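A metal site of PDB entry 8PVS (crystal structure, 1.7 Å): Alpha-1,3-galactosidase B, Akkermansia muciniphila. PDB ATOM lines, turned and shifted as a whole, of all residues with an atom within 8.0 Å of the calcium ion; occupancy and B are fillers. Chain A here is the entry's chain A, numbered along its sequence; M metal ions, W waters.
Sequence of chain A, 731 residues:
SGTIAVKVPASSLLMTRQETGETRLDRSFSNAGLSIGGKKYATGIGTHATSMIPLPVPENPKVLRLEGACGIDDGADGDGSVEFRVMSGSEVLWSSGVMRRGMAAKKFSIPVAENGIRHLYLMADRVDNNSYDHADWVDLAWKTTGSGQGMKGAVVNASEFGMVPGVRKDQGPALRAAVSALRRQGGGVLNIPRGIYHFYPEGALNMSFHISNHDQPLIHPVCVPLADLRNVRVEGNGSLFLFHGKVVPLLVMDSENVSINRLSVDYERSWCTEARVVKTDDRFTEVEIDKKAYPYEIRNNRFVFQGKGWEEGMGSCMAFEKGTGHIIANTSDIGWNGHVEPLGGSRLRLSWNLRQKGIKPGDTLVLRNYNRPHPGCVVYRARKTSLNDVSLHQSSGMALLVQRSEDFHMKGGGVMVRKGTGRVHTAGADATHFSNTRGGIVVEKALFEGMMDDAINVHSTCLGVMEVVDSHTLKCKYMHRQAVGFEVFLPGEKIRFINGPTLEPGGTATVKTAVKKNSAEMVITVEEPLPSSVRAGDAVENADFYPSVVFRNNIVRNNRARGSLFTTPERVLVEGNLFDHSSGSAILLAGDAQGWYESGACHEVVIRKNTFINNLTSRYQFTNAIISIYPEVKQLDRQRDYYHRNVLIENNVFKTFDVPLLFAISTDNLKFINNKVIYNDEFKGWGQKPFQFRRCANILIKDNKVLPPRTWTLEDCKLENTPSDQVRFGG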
ATOM      1  N   GLU A  19       4.397  18.884 -11.015  1.00  0.00           N
ATOM      2  CA  GLU A  19       5.367  19.662 -10.238  1.00  0.00           C
ATOM      3  C   GLU A  19       5.726  18.975  -8.925  1.00  0.00           C
ATOM      4  O   GLU A  19       6.848  19.167  -8.423  1.00  0.00           O
ATOM      5  CB  GLU A  19       4.800  21.074  -9.989  1.00  0.00           C
ATOM      6  CG  GLU A  19       5.704  21.991  -9.178  1.00  0.00           C
ATOM      7  CD  GLU A  19       5.163  23.420  -9.057  1.00  0.00           C
ATOM      8  OE1 GLU A  19       4.028  23.699  -9.517  1.00  0.00           O
ATOM      9  OE2 GLU A  19       5.879  24.256  -8.464  1.00  0.00           O
ATOM     10  N   HIS A  48      -1.634  17.195  -9.660  1.00  0.00           N
ATOM     11  CA  HIS A  48      -1.303  18.314  -8.784  1.00  0.00           C
ATOM     12  C   HIS A  48      -0.707  19.393  -9.668  1.00  0.00           C
ATOM     13  O   HIS A  48       0.162  19.092 -10.498  1.00  0.00           O
ATOM     14  CB  HIS A  48      -0.300  17.893  -7.681  1.00  0.00           C
ATOM     15  CG  HIS A  48      -0.219  18.865  -6.528  1.00  0.00           C
ATOM     16  ND1 HIS A  48       0.195  20.165  -6.687  1.00  0.00           N
ATOM     17  CD2 HIS A  48      -0.475  18.708  -5.217  1.00  0.00           C
ATOM     18  CE1 HIS A  48       0.172  20.785  -5.512  1.00  0.00           C
ATOM     19  NE2 HIS A  48      -0.215  19.923  -4.603  1.00  0.00           N
ATOM     20  N   ALA A  49      -1.150  20.637  -9.505  1.00  0.00           N
ATOM     21  CA  ALA A  49      -0.582  21.693 -10.337  1.00  0.00           C
ATOM     22  C   ALA A  49       0.844  22.010  -9.888  1.00  0.00           C
ATOM     23  O   ALA A  49       1.208  21.814  -8.728  1.00  0.00           O
ATOM     24  CB  ALA A  49      -1.446  22.947 -10.265  1.00  0.00           C
ATOM     25  N   THR A  50       1.679  22.473 -10.823  1.00  0.00           N
ATOM     26  CA  THR A  50       1.410  22.571 -12.248  1.00  0.00           C
ATOM     27  C   THR A  50       1.672  21.218 -12.885  1.00  0.00           C
ATOM     28  O   THR A  50       2.669  20.576 -12.588  1.00  0.00           O
ATOM     29  CB  THR A  50       2.295  23.661 -12.900  1.00  0.00           C
ATOM     30  OG1 THR A  50       1.776  24.944 -12.559  1.00  0.00           O
ATOM     31  CG2 THR A  50       2.381  23.499 -14.469  1.00  0.00           C
ATOM     32  N   ILE A  72     -10.853  21.201  -7.818  1.00  0.00           N
ATOM     33  CA  ILE A  72      -9.914  20.981  -6.718  1.00  0.00           C
ATOM     34  C   ILE A  72     -10.381  19.803  -5.882  1.00  0.00           C
ATOM     35  O   ILE A  72     -11.552  19.731  -5.482  1.00  0.00           O
ATOM     36  CB  ILE A  72      -9.792  22.239  -5.843  1.00  0.00           C
ATOM     37  CG1 ILE A  72      -9.325  23.441  -6.670  1.00  0.00           C
ATOM     38  CG2 ILE A  72      -8.848  21.961  -4.645  1.00  0.00           C
ATOM     39  CD1 ILE A  72      -8.029  23.224  -7.386  1.00  0.00           C
ATOM     40  N   ASP A  79      -6.781  25.646   0.852  1.00  0.00           N
ATOM     41  CA  ASP A  79      -7.570  26.154  -0.272  1.00  0.00           C
ATOM     42  C   ASP A  79      -6.653  26.435  -1.468  1.00  0.00           C
ATOM     43  O   ASP A  79      -6.108  27.529  -1.624  1.00  0.00           O
ATOM     44  CB  ASP A  79      -8.350  27.397   0.128  1.00  0.00           C
ATOM     45  CG  ASP A  79      -9.404  27.786  -0.914  1.00  0.00           C
ATOM     46  OD1 ASP A  79      -9.422  27.212  -2.038  1.00  0.00           O
ATOM     47  OD2 ASP A  79     -10.239  28.676  -0.584  1.00  0.00           O
ATOM     48  N   GLY A  80      -6.464  25.433  -2.326  1.00  0.00           N
ATOM     49  CA  GLY A  80      -5.620  25.614  -3.483  1.00  0.00           C
ATOM     50  C   GLY A  80      -6.293  26.477  -4.558  1.00  0.00           C
ATOM     51  O   GLY A  80      -7.415  26.963  -4.409  1.00  0.00           O
ATOM     52  N   SER A  81      -5.578  26.653  -5.670  1.00  0.00           N
ATOM     53  CA  SER A  81      -6.066  27.495  -6.755  1.00  0.00           C
ATOM     54  C   SER A  81      -5.449  26.987  -8.043  1.00  0.00           C
ATOM     55  O   SER A  81      -4.231  26.999  -8.184  1.00  0.00           O
ATOM     56  CB  SER A  81      -5.693  28.969  -6.538  1.00  0.00           C
ATOM     57  OG  SER A  81      -4.308  29.063  -6.217  1.00  0.00           O
ATOM     58  N   VAL A  82      -6.286  26.539  -8.982  1.00  0.00           N
ATOM     59  CA  VAL A  82      -5.790  25.903 -10.194  1.00  0.00           C
ATOM     60  C   VAL A  82      -6.601  26.405 -11.362  1.00  0.00           C
ATOM     61  O   VAL A  82      -7.827  26.545 -11.267  1.00  0.00           O
ATOM     62  CB  VAL A  82      -5.876  24.359 -10.101  1.00  0.00           C
ATOM     63  CG1 VAL A  82      -5.490  23.702 -11.456  1.00  0.00           C
ATOM     64  CG2 VAL A  82      -4.971  23.864  -8.984  1.00  0.00           C
ATOM     65  N   GLU A  83      -5.937  26.683 -12.479  1.00  0.00           N
ATOM     66  CA  GLU A  83      -6.617  26.940 -13.739  1.00  0.00           C
ATOM     67  C   GLU A  83      -6.410  25.731 -14.634  1.00  0.00           C
ATOM     68  O   GLU A  83      -5.269  25.384 -14.960  1.00  0.00           O
ATOM     69  CB  GLU A  83      -6.101  28.202 -14.431  1.00  0.00           C
ATOM     70  CG  GLU A  83      -6.892  28.500 -15.732  1.00  0.00           C
ATOM     71  CD  GLU A  83      -6.111  29.334 -16.717  1.00  0.00           C
ATOM     72  OE1 GLU A  83      -5.096  29.944 -16.310  1.00  0.00           O
ATOM     73  OE2 GLU A  83      -6.490  29.360 -17.913  1.00  0.00           O
ATOM     74  N   VAL A  98      -9.946  30.288 -12.656  1.00  0.00           N
ATOM     75  CA  VAL A  98      -9.305  29.840 -11.422  1.00  0.00           C
ATOM     76  C   VAL A  98     -10.307  29.060 -10.574  1.00  0.00           C
ATOM     77  O   VAL A  98     -11.335  29.605 -10.171  1.00  0.00           O
ATOM     78  CB  VAL A  98      -8.717  31.019 -10.627  1.00  0.00           C
ATOM     79  CG1 VAL A  98      -8.080  30.488  -9.347  1.00  0.00           C
ATOM     80  CG2 VAL A  98      -7.680  31.776 -11.461  1.00  0.00           C
ATOM     81  N   MET A  99      -9.999  27.812 -10.268  1.00  0.00           N
ATOM     82  CA  MET A  99     -10.869  27.011  -9.420  1.00  0.00           C
ATOM     83  C   MET A  99     -10.290  26.847  -8.024  1.00  0.00           C
ATOM     84  O   MET A  99      -9.078  26.677  -7.863  1.00  0.00           O
ATOM     85  CB  MET A  99     -11.115  25.644 -10.045  1.00  0.00           C
ATOM     86  CG  MET A  99     -11.797  25.754 -11.378  1.00  0.00           C
ATOM     87  SD  MET A  99     -12.479  24.181 -11.811  1.00  0.00           S
ATOM     88  CE  MET A  99     -13.843  24.010 -10.660  1.00  0.00           C
ATOM     89  N   ARG A 100     -11.167  26.850  -7.035  1.00  0.00           N
ATOM     90  CA  ARG A 100     -10.776  26.798  -5.626  1.00  0.00           C
ATOM     91  C   ARG A 100     -11.432  25.596  -4.952  1.00  0.00           C
ATOM     92  O   ARG A 100     -12.420  25.058  -5.447  1.00  0.00           O
ATOM     93  CB  ARG A 100     -11.192  28.061  -4.841  1.00  0.00           C
ATOM     94  CG  ARG A 100     -10.747  29.386  -5.460  1.00  0.00           C
ATOM     95  CD  ARG A 100      -9.254  29.435  -5.581  1.00  0.00           C
ATOM     96  NE  ARG A 100      -8.588  29.295  -4.288  1.00  0.00           N
ATOM     97  CZ  ARG A 100      -8.191  30.309  -3.541  1.00  0.00           C
ATOM     98  NH1 ARG A 100      -8.368  31.565  -3.916  1.00  0.00           N
ATOM     99  NH2 ARG A 100      -7.589  30.056  -2.376  1.00  0.00           N
ATOM    100  N   ASP A 125      -2.730  24.563 -14.213  1.00  0.00           N
ATOM    101  CA  ASP A 125      -1.729  25.591 -13.928  1.00  0.00           C
ATOM    102  C   ASP A 125      -1.869  26.078 -12.498  1.00  0.00           C
ATOM    103  O   ASP A 125      -2.984  26.352 -12.022  1.00  0.00           O
ATOM    104  CB  ASP A 125      -1.863  26.752 -14.897  1.00  0.00           C
ATOM    105  CG  ASP A 125      -0.740  27.742 -14.741  1.00  0.00           C
ATOM    106  OD1 ASP A 125       0.337  27.518 -15.331  1.00  0.00           O
ATOM    107  OD2 ASP A 125      -0.930  28.711 -13.985  1.00  0.00           O
ATOM    108  N   ARG A 126      -0.726  26.253 -11.819  1.00  0.00           N
ATOM    109  CA  ARG A 126      -0.738  26.601 -10.389  1.00  0.00           C
ATOM    110  C   ARG A 126      -1.270  28.014 -10.117  1.00  0.00           C
ATOM    111  O   ARG A 126      -1.624  28.301  -8.974  1.00  0.00           O
ATOM    112  CB  ARG A 126       0.667  26.483  -9.786  1.00  0.00           C
ATOM    113  CG  ARG A 126       1.610  27.600 -10.238  1.00  0.00           C
ATOM    114  CD  ARG A 126       3.060  27.145 -10.423  1.00  0.00           C
ATOM    115  NE  ARG A 126       3.680  26.574  -9.221  1.00  0.00           N
ATOM    116  CZ  ARG A 126       4.343  27.287  -8.318  1.00  0.00           C
ATOM    117  NH1 ARG A 126       4.456  28.609  -8.421  1.00  0.00           N
ATOM    118  NH2 ARG A 126       4.899  26.667  -7.267  1.00  0.00           N
ATOM    119  N   VAL A 127      -1.327  28.892 -11.121  1.00  0.00           N
ATOM    120  CA  VAL A 127      -1.807  30.276 -10.984  1.00  0.00           C
ATOM    121  C   VAL A 127      -0.807  31.140 -10.227  1.00  0.00           C
ATOM    122  O   VAL A 127      -0.256  32.088 -10.780  1.00  0.00           O
ATOM    123  CB  VAL A 127      -3.193  30.357 -10.316  1.00  0.00           C
ATOM    124  CG1 VAL A 127      -3.657  31.841 -10.238  1.00  0.00           C
ATOM    125  CG2 VAL A 127      -4.218  29.536 -11.083  1.00  0.00           C
ATOM    126  N   ASP A 128      -0.590  30.836  -8.939  1.00  0.00           N
ATOM    127  CA  ASP A 128       0.177  31.710  -8.048  1.00  0.00           C
ATOM    128  C   ASP A 128       1.337  30.938  -7.441  1.00  0.00           C
ATOM    129  O   ASP A 128       2.494  31.139  -7.838  1.00  0.00           O
ATOM    130  CB  ASP A 128      -0.761  32.269  -6.983  1.00  0.00           C
ATOM    131  CG  ASP A 128      -1.887  31.278  -6.591  1.00  0.00           C
ATOM    132  OD1 ASP A 128      -1.589  30.081  -6.388  1.00  0.00           O
ATOM    133  OD2 ASP A 128      -3.076  31.680  -6.499  1.00  0.00           O
ATOM    134  N   ASN A 129       1.065  30.065  -6.478  1.00  0.00           N
ATOM    135  CA  ASN A 129       1.985  29.014  -6.063  1.00  0.00           C
ATOM    136  C   ASN A 129       1.196  27.704  -6.150  1.00  0.00           C
ATOM    137  O   ASN A 129       0.015  27.713  -6.501  1.00  0.00           O
ATOM    138  CB  ASN A 129       2.516  29.278  -4.648  1.00  0.00           C
ATOM    139  CG  ASN A 129       1.411  29.439  -3.664  1.00  0.00           C
ATOM    140  OD1 ASN A 129       0.610  28.523  -3.462  1.00  0.00           O
ATOM    141  ND2 ASN A 129       1.344  30.604  -3.047  1.00  0.00           N
ATOM    142  N   ASN A 130       1.827  26.573  -5.851  1.00  0.00           N
ATOM    143  CA  ASN A 130       1.129  25.306  -5.995  1.00  0.00           C
ATOM    144  C   ASN A 130       0.684  24.710  -4.662  1.00  0.00           C
ATOM    145  O   ASN A 130       0.268  23.546  -4.623  1.00  0.00           O
ATOM    146  CB  ASN A 130       1.970  24.312  -6.823  1.00  0.00           C
ATOM    147  CG  ASN A 130       3.160  23.703  -6.046  1.00  0.00           C
ATOM    148  OD1 ASN A 130       3.698  24.293  -5.103  1.00  0.00           O
ATOM    149  ND2 ASN A 130       3.587  22.502  -6.490  1.00  0.00           N
ATOM    150  N   SER A 131       0.708  25.486  -3.566  1.00  0.00           N
ATOM    151  CA  SER A 131       0.226  24.991  -2.283  1.00  0.00           C
ATOM    152  C   SER A 131      -1.240  24.554  -2.348  1.00  0.00           C
ATOM    153  O   SER A 131      -2.130  25.367  -2.635  1.00  0.00           O
ATOM    154  CB  SER A 131       0.405  26.068  -1.212  1.00  0.00           C
ATOM    155  OG  SER A 131       1.772  26.406  -1.071  1.00  0.00           O
ATOM    156  N   TYR A 132      -1.490  23.275  -2.054  1.00  0.00           N
ATOM    157  CA  TYR A 132      -2.822  22.687  -1.953  1.00  0.00           C
ATOM    158  C   TYR A 132      -3.505  22.544  -3.308  1.00  0.00           C
ATOM    159  O   TYR A 132      -4.725  22.365  -3.373  1.00  0.00           O
ATOM    160  CB  TYR A 132      -3.725  23.482  -1.000  1.00  0.00           C
ATOM    161  CG  TYR A 132      -3.056  23.701   0.349  1.00  0.00           C
ATOM    162  CD1 TYR A 132      -2.719  22.615   1.161  1.00  0.00           C
ATOM    163  CD2 TYR A 132      -2.734  24.976   0.786  1.00  0.00           C
ATOM    164  CE1 TYR A 132      -2.075  22.792   2.388  1.00  0.00           C
ATOM    165  CE2 TYR A 132      -2.098  25.172   2.032  1.00  0.00           C
ATOM    166  CZ  TYR A 132      -1.780  24.083   2.831  1.00  0.00           C
ATOM    167  OH  TYR A 132      -1.140  24.246   4.058  1.00  0.00           O
ATOM    168  N   ASP A 133      -2.735  22.614  -4.379  1.00  0.00           N
ATOM    169  CA  ASP A 133      -3.312  22.539  -5.728  1.00  0.00           C
ATOM    170  C   ASP A 133      -3.550  21.082  -6.132  1.00  0.00           C
ATOM    171  O   ASP A 133      -3.056  20.648  -7.172  1.00  0.00           O
ATOM    172  CB  ASP A 133      -2.370  23.230  -6.737  1.00  0.00           C
ATOM    173  CG  ASP A 133      -2.420  24.741  -6.657  1.00  0.00           C
ATOM    174  OD1 ASP A 133      -3.211  25.277  -5.850  1.00  0.00           O
ATOM    175  OD2 ASP A 133      -1.668  25.400  -7.415  1.00  0.00           O
ATOM    176  N   HIS A 134      -4.291  20.330  -5.312  1.00  0.00           N
ATOM    177  CA  HIS A 134      -4.686  18.983  -5.710  1.00  0.00           C
ATOM    178  C   HIS A 134      -5.717  19.110  -6.816  1.00  0.00           C
ATOM    179  O   HIS A 134      -6.813  19.626  -6.585  1.00  0.00           O
ATOM    180  CB  HIS A 134      -5.298  18.227  -4.521  1.00  0.00           C
ATOM    181  CG  HIS A 134      -4.362  18.051  -3.363  1.00  0.00           C
ATOM    182  ND1 HIS A 134      -4.499  17.032  -2.451  1.00  0.00           N
ATOM    183  CD2 HIS A 134      -3.292  18.779  -2.947  1.00  0.00           C
ATOM    184  CE1 HIS A 134      -3.562  17.127  -1.521  1.00  0.00           C
ATOM    185  NE2 HIS A 134      -2.804  18.179  -1.809  1.00  0.00           N
HETATM  186 CA    CA M   1      -2.326  27.658  -6.771  1.00  0.00          CA
HETATM  187  O   HOH W   1      -2.021  27.642  -4.383  1.00  0.00           O
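The backbone NH of Arg 126 is in hydrogen-bond range of the side-chain hydroxyl of Thr 50 (2.9 Å).
OD1 of Asn 129 lies within hydrogen-bond range of N of Ser 131 (3.0 Å).
OE2 of Glu 19 is in salt-bridge range of NH2 of Arg 126, at 2.9 Å.
The backbone carbonyl oxygen (O) of Asp 133 lies within hydrogen-bond range of a ring nitrogen (ND1) of His 48 (3.3 Å).
The backbone carbonyl oxygen (O) of Asp 133 sits at hydrogen-bond distance from the backbone NH (N) of Ala 49, 3.0 Å away.
The guanidinium group (NH2) of Arg 126 lies within hydrogen-bond range of the side-chain amide oxygen (OD1) of Asn 130 (3.4 Å).
Five residues have an atom within 4 Å of the calcium ion: Ser 81, Arg 126, Asp 128, Asn 129 and Asp 133.
The calcium ion is bound by the backbone carbonyl oxygen (O) of Asn 129 (2.4 Å), the backbone carbonyl oxygen (O) of Arg 126 (2.4 Å), water W1 (2.4 Å), the side-chain carboxylate (OD2) of Asp 133 (2.4 Å), the backbone carbonyl oxygen (O) of Ser 81 (2.5 Å), the side-chain hydroxyl (OG) of Ser 81 (2.5 Å), the side-chain carboxylate (OD1) of Asp 128 (2.6 Å) and the side-chain carboxylate (OD1) of Asp 133 (2.7 Å).
Water W1 bridges O of Ser 131 and OD1 of Asn 129.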
